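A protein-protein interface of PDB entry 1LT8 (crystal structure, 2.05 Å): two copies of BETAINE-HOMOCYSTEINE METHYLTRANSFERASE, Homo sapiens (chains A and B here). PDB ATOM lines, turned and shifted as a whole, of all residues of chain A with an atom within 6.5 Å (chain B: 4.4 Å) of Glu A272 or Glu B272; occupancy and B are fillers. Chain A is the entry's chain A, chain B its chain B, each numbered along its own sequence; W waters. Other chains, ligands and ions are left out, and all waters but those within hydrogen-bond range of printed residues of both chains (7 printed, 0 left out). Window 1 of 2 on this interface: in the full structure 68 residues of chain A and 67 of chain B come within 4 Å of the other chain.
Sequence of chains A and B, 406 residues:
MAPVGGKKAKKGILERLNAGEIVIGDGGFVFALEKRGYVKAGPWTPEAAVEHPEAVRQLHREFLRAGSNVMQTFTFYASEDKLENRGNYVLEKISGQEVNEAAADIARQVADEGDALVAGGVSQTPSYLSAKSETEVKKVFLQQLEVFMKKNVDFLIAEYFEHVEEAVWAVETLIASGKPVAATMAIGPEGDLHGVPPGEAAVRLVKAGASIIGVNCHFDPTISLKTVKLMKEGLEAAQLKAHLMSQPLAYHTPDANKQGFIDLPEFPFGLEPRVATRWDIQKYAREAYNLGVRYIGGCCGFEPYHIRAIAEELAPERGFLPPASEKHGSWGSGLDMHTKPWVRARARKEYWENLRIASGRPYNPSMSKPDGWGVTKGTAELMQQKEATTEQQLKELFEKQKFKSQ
The backbone carbonyl oxygen of Lys A35 sits at hydrogen-bond distance from the backbone NH of Tyr B305. The side-chain hydroxyl of Tyr B305 lies within hydrogen-bond range of the side-chain carboxylate of Glu A272 (2.8 Å). The side-chain carboxylate of Glu B272 sits at hydrogen-bond distance from the side-chain hydroxyl of Tyr A305, at 2.6 Å. The backbone carbonyl oxygen of Pro B273 lies within hydrogen-bond range of the guanidinium group of Arg A361, at 2.8 Å. The guanidinium group of Arg A361 sits at hydrogen-bond distance from the backbone carbonyl oxygen of Val B275 (2.8 Å). O of Pro B273 sits close to O of Ser A359, 3.3 Å away.
NE2 of His A306 is in hydrogen-bond range of O of Ala A276, at 2.6 Å. OH of Tyr A305 lies within hydrogen-bond range of NE2 of His A306, 3.2 Å away. The side-chain hydroxyl (OG) of Ser A359 sits close to the backbone NH (N) of Arg A361, at 3.2 Å.
Among the printed residues, merely in contact across the chains: Arg A278 with Phe B269, Pro A273 with Pro B273, Phe A269 with Arg B278, Val A275 with Glu B272, Thr A277 with Glu B272, Ile A357 with Pro B273, Arg A361 with Ala B276, Ser A359 with Arg B274, Glu A272 with Val B275, Ile A357 with Gly B270, Ala A276 with Glu B272, Glu A272 with Thr B277, Arg A361 with Thr B277, Ala A358 with Pro B273, Glu A272 with Ala B276, Ala A358 with Arg B274, Glu A272 with Glu B272, Thr A277 with Phe B269, Thr A277 with Gly B270, Phe A269 with Thr B277 and Arg A361 with Arg B274.
Glu A272 touches just these residues of chain B: Glu B272, Val B275, Ala B276, Thr B277 and Tyr B305. Glu B272 touches just these residues of chain A: Glu A272 (3.8 Å), Val A275 (3.5 Å), Ala A276 (3.6 Å), Thr A277 (3.5 Å) and Tyr A305 (2.6 Å). Of the printed residues of chain B, Phe A269 touches Thr B277 (3.9 Å) and Arg B278 (3.4 Å). Printed residues of chain B within 4 Å of Ala A358: Pro B273 and Arg B274. Tyr A251 touches none of the printed residues of chain B. His A306 touches none of the printed residues of chain B. The nearest residue of chain A that does not touch Glu B272 is Arg A278 (4.4 Å). The nearest printed residue of chain B that does not touch Ser A359 is Val B275 (5.7 Å).
Of the 20 printed residues of chain A, 13 touch a printed residue of chain B. Printed residues of chain A that touch a printed residue of chain B: Lys A35, Phe A269, Glu A272, Pro A273, Val A275, Ala A276, Thr A277, Arg A278, Tyr A305, Ile A357, Ala A358, Ser A359 and Arg A361. Hydrophobic or aromatic side chains of chain A that line the printed part of chain B: Phe A269, Pro A273, Val A275, Tyr A305, Ile A357 and Ala A358. Among the printed residues, no Asp or Glu carboxylate lies within 4 Å of a Lys or Arg side-chain nitrogen of the other chain.
Phe A269 touches Arg B278, and with the chains exchanged Arg A278 touches Phe B269. Glu A272 touches Ala B276, and with the chains exchanged Ala A276 touches Glu B272. Glu A272 touches Thr B277, and with the chains exchanged Thr A277 touches Glu B272. Glu A272 touches Tyr B305, and with the chains exchanged Tyr A305 touches Glu B272. Of the 27 pairs that touch across the chains among the printed residues, 14 have their exchanged pair printed and touching as well.
Water W5 lies within hydrogen-bond range of the side-chain carboxylate of Glu A272 (2.6 Å), the backbone carbonyl oxygen of Phe A269 (2.8 Å) and the backbone NH of Arg B278 (2.9 Å). Water W2 lies within hydrogen-bond range of the backbone carbonyl oxygen of Gly B270 (2.6 Å), the backbone carbonyl oxygen of Ala A358 (2.7 Å) and the guanidinium group of Arg B274 (2.9 Å). Water W3 lies within hydrogen-bond range of O of Glu B272 (2.7 Å) and O of Glu A272 (2.7 Å). Water W7 lies within hydrogen-bond range of O of Phe B269 (2.8 Å), OE2 of Glu B272 (2.8 Å) and NE of Arg A278 (2.8 Å). Water W4 lies within hydrogen-bond range of OE2 of Glu A272 (2.8 Å) and NH1 of Arg B278 (2.8 Å). Water W6 bridges the side-chain carboxylate of Glu B272 and the guanidinium group of Arg A278.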
ATOM      1  N   LYS A  35      23.443  31.295 -29.827  1.00  0.00           N
ATOM      2  CA  LYS A  35      22.697  32.121 -28.889  1.00  0.00           C
ATOM      3  C   LYS A  35      23.320  33.484 -28.627  1.00  0.00           C
ATOM      4  O   LYS A  35      22.621  34.424 -28.258  1.00  0.00           O
ATOM      5  CB  LYS A  35      22.516  31.396 -27.554  1.00  0.00           C
ATOM      6  CG  LYS A  35      21.654  30.152 -27.635  1.00  0.00           C
ATOM      7  CD  LYS A  35      21.375  29.606 -26.249  1.00  0.00           C
ATOM      8  CE  LYS A  35      20.802  28.224 -26.327  1.00  0.00           C
ATOM      9  NZ  LYS A  35      21.786  27.288 -26.923  1.00  0.00           N
ATOM     10  N   TYR A 251      20.358  18.687 -22.973  1.00  0.00           N
ATOM     11  CA  TYR A 251      18.897  18.728 -23.064  1.00  0.00           C
ATOM     12  C   TYR A 251      18.322  17.361 -22.741  1.00  0.00           C
ATOM     13  O   TYR A 251      18.825  16.350 -23.226  1.00  0.00           O
ATOM     14  CB  TYR A 251      18.429  19.067 -24.476  1.00  0.00           C
ATOM     15  CG  TYR A 251      18.926  20.370 -25.013  1.00  0.00           C
ATOM     16  CD1 TYR A 251      18.444  21.575 -24.520  1.00  0.00           C
ATOM     17  CD2 TYR A 251      19.880  20.400 -26.034  1.00  0.00           C
ATOM     18  CE1 TYR A 251      18.896  22.781 -25.026  1.00  0.00           C
ATOM     19  CE2 TYR A 251      20.337  21.599 -26.542  1.00  0.00           C
ATOM     20  CZ  TYR A 251      19.843  22.785 -26.034  1.00  0.00           C
ATOM     21  OH  TYR A 251      20.321  23.976 -26.521  1.00  0.00           O
ATOM     22  N   GLU A 266      10.782  20.398 -31.480  1.00  0.00           N
ATOM     23  CA  GLU A 266      11.418  21.606 -30.955  1.00  0.00           C
ATOM     24  C   GLU A 266      12.851  21.892 -31.417  1.00  0.00           C
ATOM     25  O   GLU A 266      13.396  22.955 -31.112  1.00  0.00           O
ATOM     26  CB  GLU A 266      11.355  21.584 -29.422  1.00  0.00           C
ATOM     27  CG  GLU A 266       9.921  21.418 -28.861  1.00  0.00           C
ATOM     28  CD  GLU A 266       9.474  19.959 -28.672  1.00  0.00           C
ATOM     29  OE1 GLU A 266      10.229  19.019 -28.997  1.00  0.00           O
ATOM     30  OE2 GLU A 266       8.344  19.757 -28.181  1.00  0.00           O
ATOM     31  N   PRO A 268      15.622  23.264 -33.707  1.00  0.00           N
ATOM     32  CA  PRO A 268      16.584  23.557 -32.637  1.00  0.00           C
ATOM     33  C   PRO A 268      16.204  24.834 -31.879  1.00  0.00           C
ATOM     34  O   PRO A 268      16.961  25.292 -31.018  1.00  0.00           O
ATOM     35  CB  PRO A 268      17.875  23.755 -33.412  1.00  0.00           C
ATOM     36  CG  PRO A 268      17.368  24.609 -34.582  1.00  0.00           C
ATOM     37  CD  PRO A 268      16.013  23.967 -34.950  1.00  0.00           C
ATOM     38  N   PHE A 269      15.034  25.393 -32.185  1.00  0.00           N
ATOM     39  CA  PHE A 269      14.608  26.652 -31.585  1.00  0.00           C
ATOM     40  C   PHE A 269      13.606  26.648 -30.439  1.00  0.00           C
ATOM     41  O   PHE A 269      13.203  27.723 -29.974  1.00  0.00           O
ATOM     42  CB  PHE A 269      14.082  27.586 -32.682  1.00  0.00           C
ATOM     43  CG  PHE A 269      15.102  27.934 -33.713  1.00  0.00           C
ATOM     44  CD1 PHE A 269      14.794  27.837 -35.057  1.00  0.00           C
ATOM     45  CD2 PHE A 269      16.372  28.362 -33.341  1.00  0.00           C
ATOM     46  CE1 PHE A 269      15.726  28.162 -36.019  1.00  0.00           C
ATOM     47  CE2 PHE A 269      17.318  28.691 -34.305  1.00  0.00           C
ATOM     48  CZ  PHE A 269      16.993  28.591 -35.643  1.00  0.00           C
ATOM     49  N   GLY A 270      13.206  25.466 -29.982  1.00  0.00           N
ATOM     50  CA  GLY A 270      12.262  25.397 -28.883  1.00  0.00           C
ATOM     51  C   GLY A 270      12.714  24.403 -27.827  1.00  0.00           C
ATOM     52  O   GLY A 270      11.892  23.855 -27.098  1.00  0.00           O
ATOM     53  N   LEU A 271      14.025  24.176 -27.752  1.00  0.00           N
ATOM     54  CA  LEU A 271      14.607  23.228 -26.810  1.00  0.00           C
ATOM     55  C   LEU A 271      14.840  23.766 -25.404  1.00  0.00           C
ATOM     56  O   LEU A 271      15.190  22.994 -24.496  1.00  0.00           O
ATOM     57  CB  LEU A 271      15.939  22.704 -27.361  1.00  0.00           C
ATOM     58  CG  LEU A 271      15.879  22.001 -28.722  1.00  0.00           C
ATOM     59  CD1 LEU A 271      17.283  21.725 -29.210  1.00  0.00           C
ATOM     60  CD2 LEU A 271      15.072  20.714 -28.610  1.00  0.00           C
ATOM     61  N   GLU A 272      14.636  25.073 -25.227  1.00  0.00           N
ATOM     62  CA  GLU A 272      14.864  25.738 -23.947  1.00  0.00           C
ATOM     63  C   GLU A 272      14.403  25.019 -22.684  1.00  0.00           C
ATOM     64  O   GLU A 272      15.185  24.810 -21.768  1.00  0.00           O
ATOM     65  CB  GLU A 272      14.258  27.159 -23.959  1.00  0.00           C
ATOM     66  CG  GLU A 272      15.175  28.229 -24.561  1.00  0.00           C
ATOM     67  CD  GLU A 272      15.137  28.307 -26.089  1.00  0.00           C
ATOM     68  OE1 GLU A 272      14.644  27.372 -26.752  1.00  0.00           O
ATOM     69  OE2 GLU A 272      15.624  29.321 -26.629  1.00  0.00           O
ATOM     70  N   PRO A 273      13.131  24.619 -22.618  1.00  0.00           N
ATOM     71  CA  PRO A 273      12.673  23.940 -21.401  1.00  0.00           C
ATOM     72  C   PRO A 273      13.402  22.662 -21.010  1.00  0.00           C
ATOM     73  O   PRO A 273      13.373  22.263 -19.845  1.00  0.00           O
ATOM     74  CB  PRO A 273      11.188  23.702 -21.674  1.00  0.00           C
ATOM     75  CG  PRO A 273      11.111  23.627 -23.170  1.00  0.00           C
ATOM     76  CD  PRO A 273      12.057  24.705 -23.624  1.00  0.00           C
ATOM     77  N   ARG A 274      14.076  22.044 -21.974  1.00  0.00           N
ATOM     78  CA  ARG A 274      14.779  20.788 -21.747  1.00  0.00           C
ATOM     79  C   ARG A 274      16.164  20.917 -21.139  1.00  0.00           C
ATOM     80  O   ARG A 274      16.735  19.922 -20.690  1.00  0.00           O
ATOM     81  CB  ARG A 274      14.907  20.028 -23.072  1.00  0.00           C
ATOM     82  CG  ARG A 274      13.582  19.712 -23.788  1.00  0.00           C
ATOM     83  CD  ARG A 274      13.863  19.347 -25.249  1.00  0.00           C
ATOM     84  NE  ARG A 274      12.669  18.932 -25.968  1.00  0.00           N
ATOM     85  CZ  ARG A 274      12.140  17.713 -25.900  1.00  0.00           C
ATOM     86  NH1 ARG A 274      12.709  16.785 -25.144  1.00  0.00           N
ATOM     87  NH2 ARG A 274      11.030  17.427 -26.579  1.00  0.00           N
ATOM     88  N   VAL A 275      16.711  22.130 -21.135  1.00  0.00           N
ATOM     89  CA  VAL A 275      18.055  22.354 -20.619  1.00  0.00           C
ATOM     90  C   VAL A 275      18.308  21.833 -19.209  1.00  0.00           C
ATOM     91  O   VAL A 275      17.556  22.106 -18.273  1.00  0.00           O
ATOM     92  CB  VAL A 275      18.441  23.861 -20.668  1.00  0.00           C
ATOM     93  CG1 VAL A 275      19.813  24.066 -20.051  1.00  0.00           C
ATOM     94  CG2 VAL A 275      18.472  24.344 -22.119  1.00  0.00           C
ATOM     95  N   ALA A 276      19.400  21.097 -19.062  1.00  0.00           N
ATOM     96  CA  ALA A 276      19.770  20.533 -17.771  1.00  0.00           C
ATOM     97  C   ALA A 276      20.183  21.607 -16.768  1.00  0.00           C
ATOM     98  O   ALA A 276      20.778  22.610 -17.144  1.00  0.00           O
ATOM     99  CB  ALA A 276      20.927  19.547 -17.961  1.00  0.00           C
ATOM    100  N   THR A 277      19.863  21.398 -15.495  1.00  0.00           N
ATOM    101  CA  THR A 277      20.298  22.323 -14.452  1.00  0.00           C
ATOM    102  C   THR A 277      21.707  21.833 -14.106  1.00  0.00           C
ATOM    103  O   THR A 277      22.126  20.772 -14.568  1.00  0.00           O
ATOM    104  CB  THR A 277      19.483  22.193 -13.166  1.00  0.00           C
ATOM    105  OG1 THR A 277      19.619  20.853 -12.670  1.00  0.00           O
ATOM    106  CG2 THR A 277      18.012  22.521 -13.414  1.00  0.00           C
ATOM    107  N   ARG A 278      22.434  22.592 -13.297  1.00  0.00           N
ATOM    108  CA  ARG A 278      23.766  22.167 -12.910  1.00  0.00           C
ATOM    109  C   ARG A 278      23.679  20.889 -12.075  1.00  0.00           C
ATOM    110  O   ARG A 278      24.609  20.079 -12.075  1.00  0.00           O
ATOM    111  CB  ARG A 278      24.481  23.284 -12.138  1.00  0.00           C
ATOM    112  CG  ARG A 278      23.735  23.811 -10.919  1.00  0.00           C
ATOM    113  CD  ARG A 278      24.236  25.208 -10.541  1.00  0.00           C
ATOM    114  NE  ARG A 278      23.802  26.237 -11.486  1.00  0.00           N
ATOM    115  CZ  ARG A 278      24.260  27.488 -11.495  1.00  0.00           C
ATOM    116  NH1 ARG A 278      25.175  27.874 -10.613  1.00  0.00           N
ATOM    117  NH2 ARG A 278      23.791  28.365 -12.378  1.00  0.00           N
ATOM    118  N   TYR A 305      28.696  26.908 -17.137  1.00  0.00           N
ATOM    119  CA  TYR A 305      28.309  26.457 -15.811  1.00  0.00           C
ATOM    120  C   TYR A 305      28.014  24.963 -15.795  1.00  0.00           C
ATOM    121  O   TYR A 305      28.142  24.315 -14.761  1.00  0.00           O
ATOM    122  CB  TYR A 305      27.133  27.282 -15.266  1.00  0.00           C
ATOM    123  CG  TYR A 305      25.768  26.942 -15.829  1.00  0.00           C
ATOM    124  CD1 TYR A 305      24.836  26.225 -15.071  1.00  0.00           C
ATOM    125  CD2 TYR A 305      25.389  27.380 -17.094  1.00  0.00           C
ATOM    126  CE1 TYR A 305      23.549  25.964 -15.564  1.00  0.00           C
ATOM    127  CE2 TYR A 305      24.110  27.121 -17.594  1.00  0.00           C
ATOM    128  CZ  TYR A 305      23.198  26.418 -16.824  1.00  0.00           C
ATOM    129  OH  TYR A 305      21.933  26.186 -17.318  1.00  0.00           O
ATOM    130  N   HIS A 306      27.650  24.394 -16.937  1.00  0.00           N
ATOM    131  CA  HIS A 306      27.400  22.955 -16.965  1.00  0.00           C
ATOM    132  C   HIS A 306      28.739  22.213 -16.837  1.00  0.00           C
ATOM    133  O   HIS A 306      28.824  21.164 -16.195  1.00  0.00           O
ATOM    134  CB  HIS A 306      26.712  22.555 -18.267  1.00  0.00           C
ATOM    135  CG  HIS A 306      25.281  22.990 -18.360  1.00  0.00           C
ATOM    136  ND1 HIS A 306      24.789  23.695 -19.437  1.00  0.00           N
ATOM    137  CD2 HIS A 306      24.225  22.769 -17.539  1.00  0.00           C
ATOM    138  CE1 HIS A 306      23.491  23.884 -19.278  1.00  0.00           C
ATOM    139  NE2 HIS A 306      23.125  23.333 -18.137  1.00  0.00           N
ATOM    140  N   ILE A 357      12.037  20.305 -10.135  1.00  0.00           N
ATOM    141  CA  ILE A 357      11.745  21.629 -10.650  1.00  0.00           C
ATOM    142  C   ILE A 357      10.545  21.648 -11.591  1.00  0.00           C
ATOM    143  O   ILE A 357      10.307  20.692 -12.341  1.00  0.00           O
ATOM    144  CB  ILE A 357      12.996  22.215 -11.359  1.00  0.00           C
ATOM    145  CG1 ILE A 357      13.274  21.478 -12.673  1.00  0.00           C
ATOM    146  CG2 ILE A 357      14.221  22.064 -10.447  1.00  0.00           C
ATOM    147  CD1 ILE A 357      14.673  21.747 -13.236  1.00  0.00           C
ATOM    148  N   ALA A 358       9.793  22.742 -11.533  1.00  0.00           N
ATOM    149  CA  ALA A 358       8.619  22.932 -12.364  1.00  0.00           C
ATOM    150  C   ALA A 358       9.049  23.484 -13.712  1.00  0.00           C
ATOM    151  O   ALA A 358      10.043  24.218 -13.811  1.00  0.00           O
ATOM    152  CB  ALA A 358       7.648  23.895 -11.685  1.00  0.00           C
ATOM    153  N   SER A 359       8.303  23.135 -14.754  1.00  0.00           N
ATOM    154  CA  SER A 359       8.625  23.601 -16.096  1.00  0.00           C
ATOM    155  C   SER A 359       8.187  25.042 -16.287  1.00  0.00           C
ATOM    156  O   SER A 359       8.734  25.750 -17.126  1.00  0.00           O
ATOM    157  CB  SER A 359       7.931  22.729 -17.144  1.00  0.00           C
ATOM    158  OG  SER A 359       6.536  22.990 -17.168  1.00  0.00           O
ATOM    159  N   ARG A 361       5.472  25.939 -17.542  1.00  0.00           N
ATOM    160  CA  ARG A 361       4.617  25.985 -18.732  1.00  0.00           C
ATOM    161  C   ARG A 361       3.490  24.954 -18.595  1.00  0.00           C
ATOM    162  O   ARG A 361       3.500  23.899 -19.248  1.00  0.00           O
ATOM    163  CB  ARG A 361       5.441  25.683 -20.000  1.00  0.00           C
ATOM    164  CG  ARG A 361       6.458  26.776 -20.435  1.00  0.00           C
ATOM    165  CD  ARG A 361       6.950  26.471 -21.870  1.00  0.00           C
ATOM    166  NE  ARG A 361       7.770  27.506 -22.495  1.00  0.00           N
ATOM    167  CZ  ARG A 361       9.028  27.804 -22.167  1.00  0.00           C
ATOM    168  NH1 ARG A 361       9.670  28.759 -22.835  1.00  0.00           N
ATOM    169  NH2 ARG A 361       9.656  27.167 -21.180  1.00  0.00           N
ATOM    170  N   PHE B 269      18.683  28.356  -8.926  1.00  0.00           N
ATOM    171  CA  PHE B 269      19.414  27.279  -9.580  1.00  0.00           C
ATOM    172  C   PHE B 269      18.650  26.218 -10.371  1.00  0.00           C
ATOM    173  O   PHE B 269      19.270  25.367 -11.001  1.00  0.00           O
ATOM    174  CB  PHE B 269      20.300  26.580  -8.545  1.00  0.00           C
ATOM    175  CG  PHE B 269      21.364  27.470  -7.967  1.00  0.00           C
ATOM    176  CD1 PHE B 269      21.568  27.527  -6.591  1.00  0.00           C
ATOM    177  CD2 PHE B 269      22.184  28.226  -8.799  1.00  0.00           C
ATOM    178  CE1 PHE B 269      22.584  28.327  -6.050  1.00  0.00           C
ATOM    179  CE2 PHE B 269      23.196  29.024  -8.270  1.00  0.00           C
ATOM    180  CZ  PHE B 269      23.397  29.074  -6.888  1.00  0.00           C
ATOM    181  N   GLY B 270      17.322  26.259 -10.344  1.00  0.00           N
ATOM    182  CA  GLY B 270      16.555  25.275 -11.089  1.00  0.00           C
ATOM    183  C   GLY B 270      15.530  25.927 -11.990  1.00  0.00           C
ATOM    184  O   GLY B 270      14.480  25.348 -12.269  1.00  0.00           O
ATOM    185  N   LEU B 271      15.847  27.137 -12.442  1.00  0.00           N
ATOM    186  CA  LEU B 271      14.966  27.927 -13.290  1.00  0.00           C
ATOM    187  C   LEU B 271      15.035  27.566 -14.772  1.00  0.00           C
ATOM    188  O   LEU B 271      14.186  28.001 -15.554  1.00  0.00           O
ATOM    189  CB  LEU B 271      15.287  29.427 -13.123  1.00  0.00           C
ATOM    190  CG  LEU B 271      15.098  30.030 -11.724  1.00  0.00           C
ATOM    191  CD1 LEU B 271      15.582  31.476 -11.715  1.00  0.00           C
ATOM    192  CD2 LEU B 271      13.621  29.971 -11.319  1.00  0.00           C
ATOM    193  N   GLU B 272      16.038  26.775 -15.148  1.00  0.00           N
ATOM    194  CA  GLU B 272      16.246  26.388 -16.544  1.00  0.00           C
ATOM    195  C   GLU B 272      15.024  26.111 -17.418  1.00  0.00           C
ATOM    196  O   GLU B 272      14.884  26.700 -18.479  1.00  0.00           O
ATOM    197  CB  GLU B 272      17.182  25.177 -16.635  1.00  0.00           C
ATOM    198  CG  GLU B 272      18.667  25.507 -16.637  1.00  0.00           C
ATOM    199  CD  GLU B 272      19.216  25.838 -15.253  1.00  0.00           C
ATOM    200  OE1 GLU B 272      18.434  25.889 -14.276  1.00  0.00           O
ATOM    201  OE2 GLU B 272      20.443  26.049 -15.148  1.00  0.00           O
ATOM    202  N   PRO B 273      14.120  25.219 -16.983  1.00  0.00           N
ATOM    203  CA  PRO B 273      12.928  24.895 -17.782  1.00  0.00           C
ATOM    204  C   PRO B 273      12.027  26.069 -18.166  1.00  0.00           C
ATOM    205  O   PRO B 273      11.336  26.026 -19.186  1.00  0.00           O
ATOM    206  CB  PRO B 273      12.174  23.894 -16.897  1.00  0.00           C
ATOM    207  CG  PRO B 273      13.251  23.305 -16.036  1.00  0.00           C
ATOM    208  CD  PRO B 273      14.098  24.496 -15.702  1.00  0.00           C
ATOM    209  N   ARG B 274      12.049  27.110 -17.346  1.00  0.00           N
ATOM    210  CA  ARG B 274      11.206  28.283 -17.534  1.00  0.00           C
ATOM    211  C   ARG B 274      11.673  29.280 -18.572  1.00  0.00           C
ATOM    212  O   ARG B 274      10.911  30.158 -18.971  1.00  0.00           O
ATOM    213  CB  ARG B 274      11.046  29.012 -16.190  1.00  0.00           C
ATOM    214  CG  ARG B 274      10.475  28.164 -15.058  1.00  0.00           C
ATOM    215  CD  ARG B 274      10.767  28.839 -13.719  1.00  0.00           C
ATOM    216  NE  ARG B 274      10.198  28.137 -12.576  1.00  0.00           N
ATOM    217  CZ  ARG B 274       8.925  28.214 -12.196  1.00  0.00           C
ATOM    218  NH1 ARG B 274       8.060  28.973 -12.872  1.00  0.00           N
ATOM    219  NH2 ARG B 274       8.517  27.536 -11.126  1.00  0.00           N
ATOM    220  N   VAL B 275      12.916  29.161 -19.015  1.00  0.00           N
ATOM    221  CA  VAL B 275      13.437  30.114 -19.986  1.00  0.00           C
ATOM    222  C   VAL B 275      12.599  30.224 -21.258  1.00  0.00           C
ATOM    223  O   VAL B 275      12.231  29.223 -21.878  1.00  0.00           O
ATOM    224  CB  VAL B 275      14.894  29.789 -20.371  1.00  0.00           C
ATOM    225  CG1 VAL B 275      15.364  30.739 -21.468  1.00  0.00           C
ATOM    226  CG2 VAL B 275      15.797  29.926 -19.139  1.00  0.00           C
ATOM    227  N   ALA B 276      12.322  31.465 -21.648  1.00  0.00           N
ATOM    228  CA  ALA B 276      11.538  31.729 -22.840  1.00  0.00           C
ATOM    229  C   ALA B 276      12.308  31.432 -24.120  1.00  0.00           C
ATOM    230  O   ALA B 276      13.527  31.594 -24.184  1.00  0.00           O
ATOM    231  CB  ALA B 276      11.075  33.187 -22.845  1.00  0.00           C
ATOM    232  N   THR B 277      11.590  30.979 -25.139  1.00  0.00           N
ATOM    233  CA  THR B 277      12.201  30.711 -26.433  1.00  0.00           C
ATOM    234  C   THR B 277      12.253  32.081 -27.112  1.00  0.00           C
ATOM    235  O   THR B 277      11.643  33.042 -26.632  1.00  0.00           O
ATOM    236  CB  THR B 277      11.304  29.848 -27.303  1.00  0.00           C
ATOM    237  OG1 THR B 277      10.080  30.559 -27.518  1.00  0.00           O
ATOM    238  CG2 THR B 277      10.999  28.512 -26.638  1.00  0.00           C
ATOM    239  N   ARG B 278      12.963  32.172 -28.230  1.00  0.00           N
ATOM    240  CA  ARG B 278      13.013  33.436 -28.941  1.00  0.00           C
ATOM    241  C   ARG B 278      11.609  33.799 -29.416  1.00  0.00           C
ATOM    242  O   ARG B 278      11.280  34.976 -29.538  1.00  0.00           O
ATOM    243  CB  ARG B 278      13.976  33.351 -30.126  1.00  0.00           C
ATOM    244  CG  ARG B 278      13.631  32.317 -31.184  1.00  0.00           C
ATOM    245  CD  ARG B 278      14.866  32.049 -32.017  1.00  0.00           C
ATOM    246  NE  ARG B 278      15.867  31.320 -31.236  1.00  0.00           N
ATOM    247  CZ  ARG B 278      17.137  31.159 -31.595  1.00  0.00           C
ATOM    248  NH1 ARG B 278      17.963  30.471 -30.817  1.00  0.00           N
ATOM    249  NH2 ARG B 278      17.591  31.698 -32.717  1.00  0.00           N
ATOM    250  N   TYR B 305      20.306  36.365 -27.869  1.00  0.00           N
ATOM    251  CA  TYR B 305      19.292  35.999 -28.851  1.00  0.00           C
ATOM    252  C   TYR B 305      17.893  36.459 -28.447  1.00  0.00           C
ATOM    253  O   TYR B 305      17.044  36.682 -29.313  1.00  0.00           O
ATOM    254  CB  TYR B 305      19.310  34.486 -29.153  1.00  0.00           C
ATOM    255  CG  TYR B 305      18.747  33.585 -28.073  1.00  0.00           C
ATOM    256  CD1 TYR B 305      19.511  33.236 -26.960  1.00  0.00           C
ATOM    257  CD2 TYR B 305      17.452  33.073 -28.174  1.00  0.00           C
ATOM    258  CE1 TYR B 305      19.003  32.391 -25.969  1.00  0.00           C
ATOM    259  CE2 TYR B 305      16.931  32.228 -27.191  1.00  0.00           C
ATOM    260  CZ  TYR B 305      17.718  31.894 -26.090  1.00  0.00           C
ATOM    261  OH  TYR B 305      17.218  31.073 -25.099  1.00  0.00           O
HETATM  262  O   HOH W   1       9.089  24.711 -19.745  1.00  0.00           O
HETATM  263  O   HOH W   2      11.911  25.826 -12.685  1.00  0.00           O
HETATM  264  O   HOH W   3      16.560  26.796 -20.551  1.00  0.00           O
HETATM  265  O   HOH W   4      17.569  28.894 -28.552  1.00  0.00           O
HETATM  266  O   HOH W   5      14.640  29.944 -28.995  1.00  0.00           O
HETATM  267  O   HOH W   6      21.516  28.444 -14.091  1.00  0.00           O
HETATM  268  O   HOH W   7      21.442  25.250 -12.696  1.00  0.00           O
